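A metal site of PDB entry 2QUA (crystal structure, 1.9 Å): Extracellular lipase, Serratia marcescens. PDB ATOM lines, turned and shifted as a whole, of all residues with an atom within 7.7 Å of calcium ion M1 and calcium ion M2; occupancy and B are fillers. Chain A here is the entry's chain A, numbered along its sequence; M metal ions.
Of the 29 residues printed, 7 come within 4 Å of calcium ion M2. The nearest printed residue that does not touch calcium ion M2 is Asp 378 (4.2 Å).
Calcium ion M1 is bound by the backbone carbonyl oxygen (O) of Lys 414 (2.3 Å). Calcium ion M1 is bound by O of Gly 397, 2.4 Å away. Calcium ion M1 is bound by the backbone carbonyl oxygen (O) of Arg 395, at 2.4 Å. Calcium ion M1 is bound by OD2 of Asp 399 (2.4 Å). Calcium ion M1 is bound by O of Gly 412, at 2.4 Å. OD1 of Asn 417 binds calcium ion M1 (2.4 Å).
Calcium ion M2 is bound by O of Asp 396, O of Gly 394, OD2 of Asp 381, OD1 of Asp 399, O of Gly 379, O of Ser 377 and OD2 of Asp 399. Calcium ion M2 has seven donor atoms within binding distance.
Residues that only touch calcium ion M1: Gly 413 (3.97 Å). Of the 29 residues printed, 8 come within 4 Å of calcium ion M1.
The backbone carbonyl oxygen of Ala 411 is in hydrogen-bond range of the backbone NH of Gly 394 (2.8 Å). The backbone carbonyl oxygen of Asp 381 lies within hydrogen-bond range of the backbone NH of Ile 400 (2.9 Å). N of Ile 418 lies within hydrogen-bond range of O of Asp 399, 2.8 Å away. The backbone NH (N) of Gly 379 sits at hydrogen-bond distance from the side-chain hydroxyl (OG) of Ser 377. The side-chain carboxylate (OD2) of Asp 378 is in salt-bridge range of the guanidinium group (NH2) of Arg 395 (2.9 Å). O of Gly 413 lies within hydrogen-bond range of ND2 of Asn 417, at 3.0 Å. The side-chain amide nitrogen (ND2) of Asn 417 is in hydrogen-bond range of the backbone carbonyl oxygen (O) of Gly 415 (3.4 Å). The backbone carbonyl oxygen (O) of Asp 451 lies within hydrogen-bond range of the side-chain amide nitrogen (ND2) of Asn 417 (2.8 Å).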
ATOM      1  N   SER A 346     -34.406  32.153   1.623  1.00  0.00           N
ATOM      2  CA  SER A 346     -35.100  31.117   2.354  1.00  0.00           C
ATOM      3  C   SER A 346     -35.026  31.312   3.872  1.00  0.00           C
ATOM      4  O   SER A 346     -33.939  31.314   4.444  1.00  0.00           O
ATOM      5  CB  SER A 346     -34.553  29.724   1.976  1.00  0.00           C
ATOM      6  OG  SER A 346     -35.168  28.736   2.780  1.00  0.00           O
ATOM      7  N   ARG A 353     -40.232  23.668   5.720  1.00  0.00           N
ATOM      8  CA  ARG A 353     -39.054  23.618   4.822  1.00  0.00           C
ATOM      9  C   ARG A 353     -39.107  22.386   3.917  1.00  0.00           C
ATOM     10  O   ARG A 353     -38.696  22.448   2.760  1.00  0.00           O
ATOM     11  CB  ARG A 353     -37.722  23.665   5.585  1.00  0.00           C
ATOM     12  CG  ARG A 353     -36.463  23.969   4.696  1.00  0.00           C
ATOM     13  CD  ARG A 353     -35.154  24.112   5.551  1.00  0.00           C
ATOM     14  NE  ARG A 353     -35.316  25.104   6.630  1.00  0.00           N
ATOM     15  CZ  ARG A 353     -35.433  24.808   7.922  1.00  0.00           C
ATOM     16  NH1 ARG A 353     -35.398  23.532   8.337  1.00  0.00           N
ATOM     17  NH2 ARG A 353     -35.592  25.783   8.814  1.00  0.00           N
ATOM     18  N   ILE A 375     -31.463  32.072  -2.439  1.00  0.00           N
ATOM     19  CA  ILE A 375     -30.469  31.685  -1.428  1.00  0.00           C
ATOM     20  C   ILE A 375     -31.028  30.708  -0.423  1.00  0.00           C
ATOM     21  O   ILE A 375     -31.907  31.087   0.357  1.00  0.00           O
ATOM     22  CB  ILE A 375     -29.982  32.917  -0.617  1.00  0.00           C
ATOM     23  CG1 ILE A 375     -29.600  34.089  -1.535  1.00  0.00           C
ATOM     24  CG2 ILE A 375     -28.839  32.527   0.302  1.00  0.00           C
ATOM     25  CD1 ILE A 375     -28.527  33.742  -2.532  1.00  0.00           C
ATOM     26  N   GLY A 376     -30.498  29.470  -0.430  1.00  0.00           N
ATOM     27  CA  GLY A 376     -30.978  28.407   0.462  1.00  0.00           C
ATOM     28  C   GLY A 376     -30.547  28.620   1.901  1.00  0.00           C
ATOM     29  O   GLY A 376     -30.030  29.668   2.274  1.00  0.00           O
ATOM     30  N   SER A 377     -30.769  27.603   2.722  1.00  0.00           N
ATOM     31  CA  SER A 377     -30.395  27.660   4.104  1.00  0.00           C
ATOM     32  C   SER A 377     -29.397  26.521   4.302  1.00  0.00           C
ATOM     33  O   SER A 377     -29.168  25.699   3.381  1.00  0.00           O
ATOM     34  CB  SER A 377     -31.647  27.441   4.980  1.00  0.00           C
ATOM     35  OG  SER A 377     -31.926  26.045   5.052  1.00  0.00           O
ATOM     36  N   ASP A 378     -28.792  26.439   5.479  1.00  0.00           N
ATOM     37  CA  ASP A 378     -27.920  25.288   5.715  1.00  0.00           C
ATOM     38  C   ASP A 378     -28.711  24.007   6.035  1.00  0.00           C
ATOM     39  O   ASP A 378     -28.123  22.983   6.328  1.00  0.00           O
ATOM     40  CB  ASP A 378     -26.874  25.614   6.783  1.00  0.00           C
ATOM     41  CG  ASP A 378     -25.794  26.563   6.247  1.00  0.00           C
ATOM     42  OD1 ASP A 378     -25.444  26.451   5.046  1.00  0.00           O
ATOM     43  OD2 ASP A 378     -25.311  27.398   7.014  1.00  0.00           O
ATOM     44  N   GLY A 379     -30.042  24.082   5.952  1.00  0.00           N
ATOM     45  CA  GLY A 379     -30.871  22.878   6.056  1.00  0.00           C
ATOM     46  C   GLY A 379     -31.197  22.309   4.676  1.00  0.00           C
ATOM     47  O   GLY A 379     -30.679  22.773   3.652  1.00  0.00           O
ATOM     48  N   ASN A 380     -32.039  21.280   4.651  1.00  0.00           N
ATOM     49  CA  ASN A 380     -32.511  20.649   3.434  1.00  0.00           C
ATOM     50  C   ASN A 380     -33.602  21.486   2.780  1.00  0.00           C
ATOM     51  O   ASN A 380     -34.717  21.605   3.301  1.00  0.00           O
ATOM     52  CB  ASN A 380     -33.098  19.267   3.745  1.00  0.00           C
ATOM     53  CG  ASN A 380     -32.066  18.319   4.297  1.00  0.00           C
ATOM     54  OD1 ASN A 380     -30.870  18.635   4.371  1.00  0.00           O
ATOM     55  ND2 ASN A 380     -32.509  17.144   4.685  1.00  0.00           N
ATOM     56  N   ASP A 381     -33.270  22.066   1.630  1.00  0.00           N
ATOM     57  CA  ASP A 381     -34.170  23.006   0.952  1.00  0.00           C
ATOM     58  C   ASP A 381     -34.861  22.427  -0.280  1.00  0.00           C
ATOM     59  O   ASP A 381     -34.341  21.486  -0.903  1.00  0.00           O
ATOM     60  CB  ASP A 381     -33.386  24.267   0.536  1.00  0.00           C
ATOM     61  CG  ASP A 381     -32.687  24.925   1.710  1.00  0.00           C
ATOM     62  OD1 ASP A 381     -33.420  25.222   2.705  1.00  0.00           O
ATOM     63  OD2 ASP A 381     -31.437  25.148   1.639  1.00  0.00           O
ATOM     64  N   LEU A 382     -36.024  22.994  -0.595  1.00  0.00           N
ATOM     65  CA  LEU A 382     -36.728  22.800  -1.863  1.00  0.00           C
ATOM     66  C   LEU A 382     -36.708  24.171  -2.525  1.00  0.00           C
ATOM     67  O   LEU A 382     -37.342  25.117  -2.062  1.00  0.00           O
ATOM     68  CB  LEU A 382     -38.166  22.309  -1.673  1.00  0.00           C
ATOM     69  CG  LEU A 382     -38.383  21.071  -0.801  1.00  0.00           C
ATOM     70  CD1 LEU A 382     -39.887  20.696  -0.718  1.00  0.00           C
ATOM     71  CD2 LEU A 382     -37.518  19.874  -1.276  1.00  0.00           C
ATOM     72  N   ILE A 383     -35.965  24.277  -3.618  1.00  0.00           N
ATOM     73  CA  ILE A 383     -35.711  25.551  -4.244  1.00  0.00           C
ATOM     74  C   ILE A 383     -36.179  25.503  -5.704  1.00  0.00           C
ATOM     75  O   ILE A 383     -35.785  24.591  -6.429  1.00  0.00           O
ATOM     76  CB  ILE A 383     -34.192  25.855  -4.163  1.00  0.00           C
ATOM     77  CG1 ILE A 383     -33.781  26.057  -2.690  1.00  0.00           C
ATOM     78  CG2 ILE A 383     -33.813  27.101  -5.011  1.00  0.00           C
ATOM     79  CD1 ILE A 383     -32.253  26.255  -2.507  1.00  0.00           C
ATOM     80  N   GLU A 393     -28.777  28.750  -4.984  1.00  0.00           N
ATOM     81  CA  GLU A 393     -27.692  28.353  -4.095  1.00  0.00           C
ATOM     82  C   GLU A 393     -28.234  27.491  -2.976  1.00  0.00           C
ATOM     83  O   GLU A 393     -28.995  27.965  -2.135  1.00  0.00           O
ATOM     84  CB  GLU A 393     -26.992  29.584  -3.504  1.00  0.00           C
ATOM     85  CG  GLU A 393     -25.734  29.219  -2.745  1.00  0.00           C
ATOM     86  CD  GLU A 393     -25.005  30.420  -2.195  1.00  0.00           C
ATOM     87  OE1 GLU A 393     -25.657  31.473  -2.010  1.00  0.00           O
ATOM     88  OE2 GLU A 393     -23.784  30.324  -1.931  1.00  0.00           O
ATOM     89  N   GLY A 394     -27.849  26.219  -2.963  1.00  0.00           N
ATOM     90  CA  GLY A 394     -28.320  25.329  -1.890  1.00  0.00           C
ATOM     91  C   GLY A 394     -27.692  25.507  -0.508  1.00  0.00           C
ATOM     92  O   GLY A 394     -28.372  25.327   0.500  1.00  0.00           O
ATOM     93  N   ARG A 395     -26.404  25.861  -0.454  1.00  0.00           N
ATOM     94  CA  ARG A 395     -25.622  25.805   0.783  1.00  0.00           C
ATOM     95  C   ARG A 395     -25.643  24.356   1.353  1.00  0.00           C
ATOM     96  O   ARG A 395     -25.927  23.407   0.636  1.00  0.00           O
ATOM     97  CB  ARG A 395     -26.104  26.853   1.822  1.00  0.00           C
ATOM     98  CG  ARG A 395     -26.116  28.308   1.298  1.00  0.00           C
ATOM     99  CD  ARG A 395     -26.495  29.307   2.407  1.00  0.00           C
ATOM    100  NE  ARG A 395     -25.782  29.029   3.648  1.00  0.00           N
ATOM    101  CZ  ARG A 395     -24.668  29.640   4.055  1.00  0.00           C
ATOM    102  NH1 ARG A 395     -24.105  30.598   3.312  1.00  0.00           N
ATOM    103  NH2 ARG A 395     -24.118  29.293   5.205  1.00  0.00           N
ATOM    104  N   ASP A 396     -25.335  24.211   2.639  1.00  0.00           N
ATOM    105  CA  ASP A 396     -25.298  22.899   3.293  1.00  0.00           C
ATOM    106  C   ASP A 396     -26.674  22.238   3.245  1.00  0.00           C
ATOM    107  O   ASP A 396     -27.680  22.853   2.887  1.00  0.00           O
ATOM    108  CB  ASP A 396     -24.854  23.007   4.760  1.00  0.00           C
ATOM    109  CG  ASP A 396     -23.397  23.415   4.916  1.00  0.00           C
ATOM    110  OD1 ASP A 396     -22.746  23.794   3.912  1.00  0.00           O
ATOM    111  OD2 ASP A 396     -22.900  23.364   6.074  1.00  0.00           O
ATOM    112  N   GLY A 397     -26.691  20.965   3.624  1.00  0.00           N
ATOM    113  CA  GLY A 397     -27.931  20.217   3.609  1.00  0.00           C
ATOM    114  C   GLY A 397     -28.190  19.614   2.250  1.00  0.00           C
ATOM    115  O   GLY A 397     -27.596  19.991   1.225  1.00  0.00           O
ATOM    116  N   ASP A 398     -29.103  18.638   2.251  1.00  0.00           N
ATOM    117  CA  ASP A 398     -29.512  17.912   1.065  1.00  0.00           C
ATOM    118  C   ASP A 398     -30.635  18.688   0.382  1.00  0.00           C
ATOM    119  O   ASP A 398     -31.774  18.706   0.830  1.00  0.00           O
ATOM    120  CB  ASP A 398     -29.988  16.508   1.461  1.00  0.00           C
ATOM    121  CG  ASP A 398     -28.906  15.687   2.142  1.00  0.00           C
ATOM    122  OD1 ASP A 398     -27.709  16.013   2.047  1.00  0.00           O
ATOM    123  OD2 ASP A 398     -29.259  14.665   2.761  1.00  0.00           O
ATOM    124  N   ASP A 399     -30.302  19.335  -0.731  1.00  0.00           N
ATOM    125  CA  ASP A 399     -31.210  20.260  -1.371  1.00  0.00           C
ATOM    126  C   ASP A 399     -31.767  19.683  -2.661  1.00  0.00           C
ATOM    127  O   ASP A 399     -31.091  18.880  -3.330  1.00  0.00           O
ATOM    128  CB  ASP A 399     -30.457  21.592  -1.615  1.00  0.00           C
ATOM    129  CG  ASP A 399     -29.962  22.219  -0.309  1.00  0.00           C
ATOM    130  OD1 ASP A 399     -30.778  22.369   0.623  1.00  0.00           O
ATOM    131  OD2 ASP A 399     -28.772  22.586  -0.160  1.00  0.00           O
ATOM    132  N   ILE A 400     -32.996  20.078  -2.995  1.00  0.00           N
ATOM    133  CA  ILE A 400     -33.608  19.704  -4.296  1.00  0.00           C
ATOM    134  C   ILE A 400     -33.938  20.982  -5.060  1.00  0.00           C
ATOM    135  O   ILE A 400     -34.569  21.882  -4.502  1.00  0.00           O
ATOM    136  CB  ILE A 400     -34.863  18.790  -4.151  1.00  0.00           C
ATOM    137  CG1 ILE A 400     -34.565  17.604  -3.241  1.00  0.00           C
ATOM    138  CG2 ILE A 400     -35.363  18.299  -5.556  1.00  0.00           C
ATOM    139  CD1 ILE A 400     -35.751  16.684  -2.945  1.00  0.00           C
ATOM    140  N   PHE A 401     -33.489  21.049  -6.323  1.00  0.00           N
ATOM    141  CA  PHE A 401     -33.791  22.138  -7.223  1.00  0.00           C
ATOM    142  C   PHE A 401     -34.708  21.742  -8.356  1.00  0.00           C
ATOM    143  O   PHE A 401     -34.605  20.626  -8.919  1.00  0.00           O
ATOM    144  CB  PHE A 401     -32.508  22.663  -7.854  1.00  0.00           C
ATOM    145  CG  PHE A 401     -31.486  23.026  -6.849  1.00  0.00           C
ATOM    146  CD1 PHE A 401     -31.375  24.336  -6.377  1.00  0.00           C
ATOM    147  CD2 PHE A 401     -30.643  22.062  -6.351  1.00  0.00           C
ATOM    148  CE1 PHE A 401     -30.421  24.677  -5.416  1.00  0.00           C
ATOM    149  CE2 PHE A 401     -29.680  22.386  -5.365  1.00  0.00           C
ATOM    150  CZ  PHE A 401     -29.585  23.698  -4.919  1.00  0.00           C
ATOM    151  N   ALA A 411     -25.747  26.099  -7.579  1.00  0.00           N
ATOM    152  CA  ALA A 411     -24.697  25.636  -6.689  1.00  0.00           C
ATOM    153  C   ALA A 411     -25.288  24.732  -5.599  1.00  0.00           C
ATOM    154  O   ALA A 411     -25.809  25.210  -4.586  1.00  0.00           O
ATOM    155  CB  ALA A 411     -23.978  26.820  -6.065  1.00  0.00           C
ATOM    156  N   GLY A 412     -25.197  23.414  -5.802  1.00  0.00           N
ATOM    157  CA  GLY A 412     -25.747  22.465  -4.817  1.00  0.00           C
ATOM    158  C   GLY A 412     -25.163  22.661  -3.422  1.00  0.00           C
ATOM    159  O   GLY A 412     -25.846  22.426  -2.398  1.00  0.00           O
ATOM    160  N   GLY A 413     -23.906  23.090  -3.372  1.00  0.00           N
ATOM    161  CA  GLY A 413     -23.188  23.184  -2.106  1.00  0.00           C
ATOM    162  C   GLY A 413     -22.916  21.815  -1.508  1.00  0.00           C
ATOM    163  O   GLY A 413     -22.963  20.782  -2.212  1.00  0.00           O
ATOM    164  N   LYS A 414     -22.631  21.773  -0.210  1.00  0.00           N
ATOM    165  CA  LYS A 414     -22.489  20.468   0.447  1.00  0.00           C
ATOM    166  C   LYS A 414     -23.780  19.646   0.451  1.00  0.00           C
ATOM    167  O   LYS A 414     -24.880  20.155   0.163  1.00  0.00           O
ATOM    168  CB  LYS A 414     -22.001  20.633   1.894  1.00  0.00           C
ATOM    169  CG  LYS A 414     -20.593  21.142   2.002  1.00  0.00           C
ATOM    170  CD  LYS A 414     -20.205  21.336   3.458  1.00  0.00           C
ATOM    171  CE  LYS A 414     -18.853  21.994   3.534  1.00  0.00           C
ATOM    172  NZ  LYS A 414     -18.421  22.127   4.933  1.00  0.00           N
ATOM    173  N   GLY A 415     -23.624  18.372   0.798  1.00  0.00           N
ATOM    174  CA  GLY A 415     -24.761  17.478   0.972  1.00  0.00           C
ATOM    175  C   GLY A 415     -25.062  16.685  -0.281  1.00  0.00           C
ATOM    176  O   GLY A 415     -24.319  16.721  -1.273  1.00  0.00           O
ATOM    177  N   HIS A 416     -26.160  15.952  -0.214  1.00  0.00           N
ATOM    178  CA  HIS A 416     -26.612  15.161  -1.339  1.00  0.00           C
ATOM    179  C   HIS A 416     -27.701  15.980  -2.054  1.00  0.00           C
ATOM    180  O   HIS A 416     -28.815  16.099  -1.570  1.00  0.00           O
ATOM    181  CB  HIS A 416     -27.135  13.800  -0.872  1.00  0.00           C
ATOM    182  CG  HIS A 416     -27.623  12.942  -1.996  1.00  0.00           C
ATOM    183  ND1 HIS A 416     -26.933  11.835  -2.442  1.00  0.00           N
ATOM    184  CD2 HIS A 416     -28.739  13.031  -2.770  1.00  0.00           C
ATOM    185  CE1 HIS A 416     -27.600  11.285  -3.449  1.00  0.00           C
ATOM    186  NE2 HIS A 416     -28.692  11.989  -3.670  1.00  0.00           N
ATOM    187  N   ASN A 417     -27.357  16.549  -3.210  1.00  0.00           N
ATOM    188  CA  ASN A 417     -28.260  17.477  -3.865  1.00  0.00           C
ATOM    189  C   ASN A 417     -28.863  16.906  -5.120  1.00  0.00           C
ATOM    190  O   ASN A 417     -28.189  16.173  -5.853  1.00  0.00           O
ATOM    191  CB  ASN A 417     -27.531  18.802  -4.177  1.00  0.00           C
ATOM    192  CG  ASN A 417     -26.764  19.332  -2.987  1.00  0.00           C
ATOM    193  OD1 ASN A 417     -27.339  19.682  -1.939  1.00  0.00           O
ATOM    194  ND2 ASN A 417     -25.439  19.401  -3.134  1.00  0.00           N
ATOM    195  N   ILE A 418     -30.139  17.218  -5.342  1.00  0.00           N
ATOM    196  CA  ILE A 418     -30.902  16.672  -6.484  1.00  0.00           C
ATOM    197  C   ILE A 418     -31.329  17.805  -7.411  1.00  0.00           C
ATOM    198  O   ILE A 418     -31.746  18.894  -6.952  1.00  0.00           O
ATOM    199  CB  ILE A 418     -32.134  15.860  -5.993  1.00  0.00           C
ATOM    200  CG1 ILE A 418     -31.685  14.675  -5.116  1.00  0.00           C
ATOM    201  CG2 ILE A 418     -33.000  15.376  -7.188  1.00  0.00           C
ATOM    202  CD1 ILE A 418     -32.782  14.057  -4.288  1.00  0.00           C
ATOM    203  N   ASP A 451     -22.218  20.157  -7.886  1.00  0.00           N
ATOM    204  CA  ASP A 451     -22.532  19.332  -6.706  1.00  0.00           C
ATOM    205  C   ASP A 451     -23.910  18.671  -6.716  1.00  0.00           C
ATOM    206  O   ASP A 451     -24.567  18.555  -5.669  1.00  0.00           O
ATOM    207  CB  ASP A 451     -22.343  20.140  -5.420  1.00  0.00           C
ATOM    208  CG  ASP A 451     -20.883  20.552  -5.242  1.00  0.00           C
ATOM    209  OD1 ASP A 451     -19.997  19.662  -5.248  1.00  0.00           O
ATOM    210  OD2 ASP A 451     -20.628  21.755  -5.133  1.00  0.00           O
HETATM  211 CA    CA M   1     -26.716  21.443  -0.417  1.00  0.00          CA
HETATM  212 CA    CA M   2     -29.505  23.864   1.914  1.00  0.00          CA
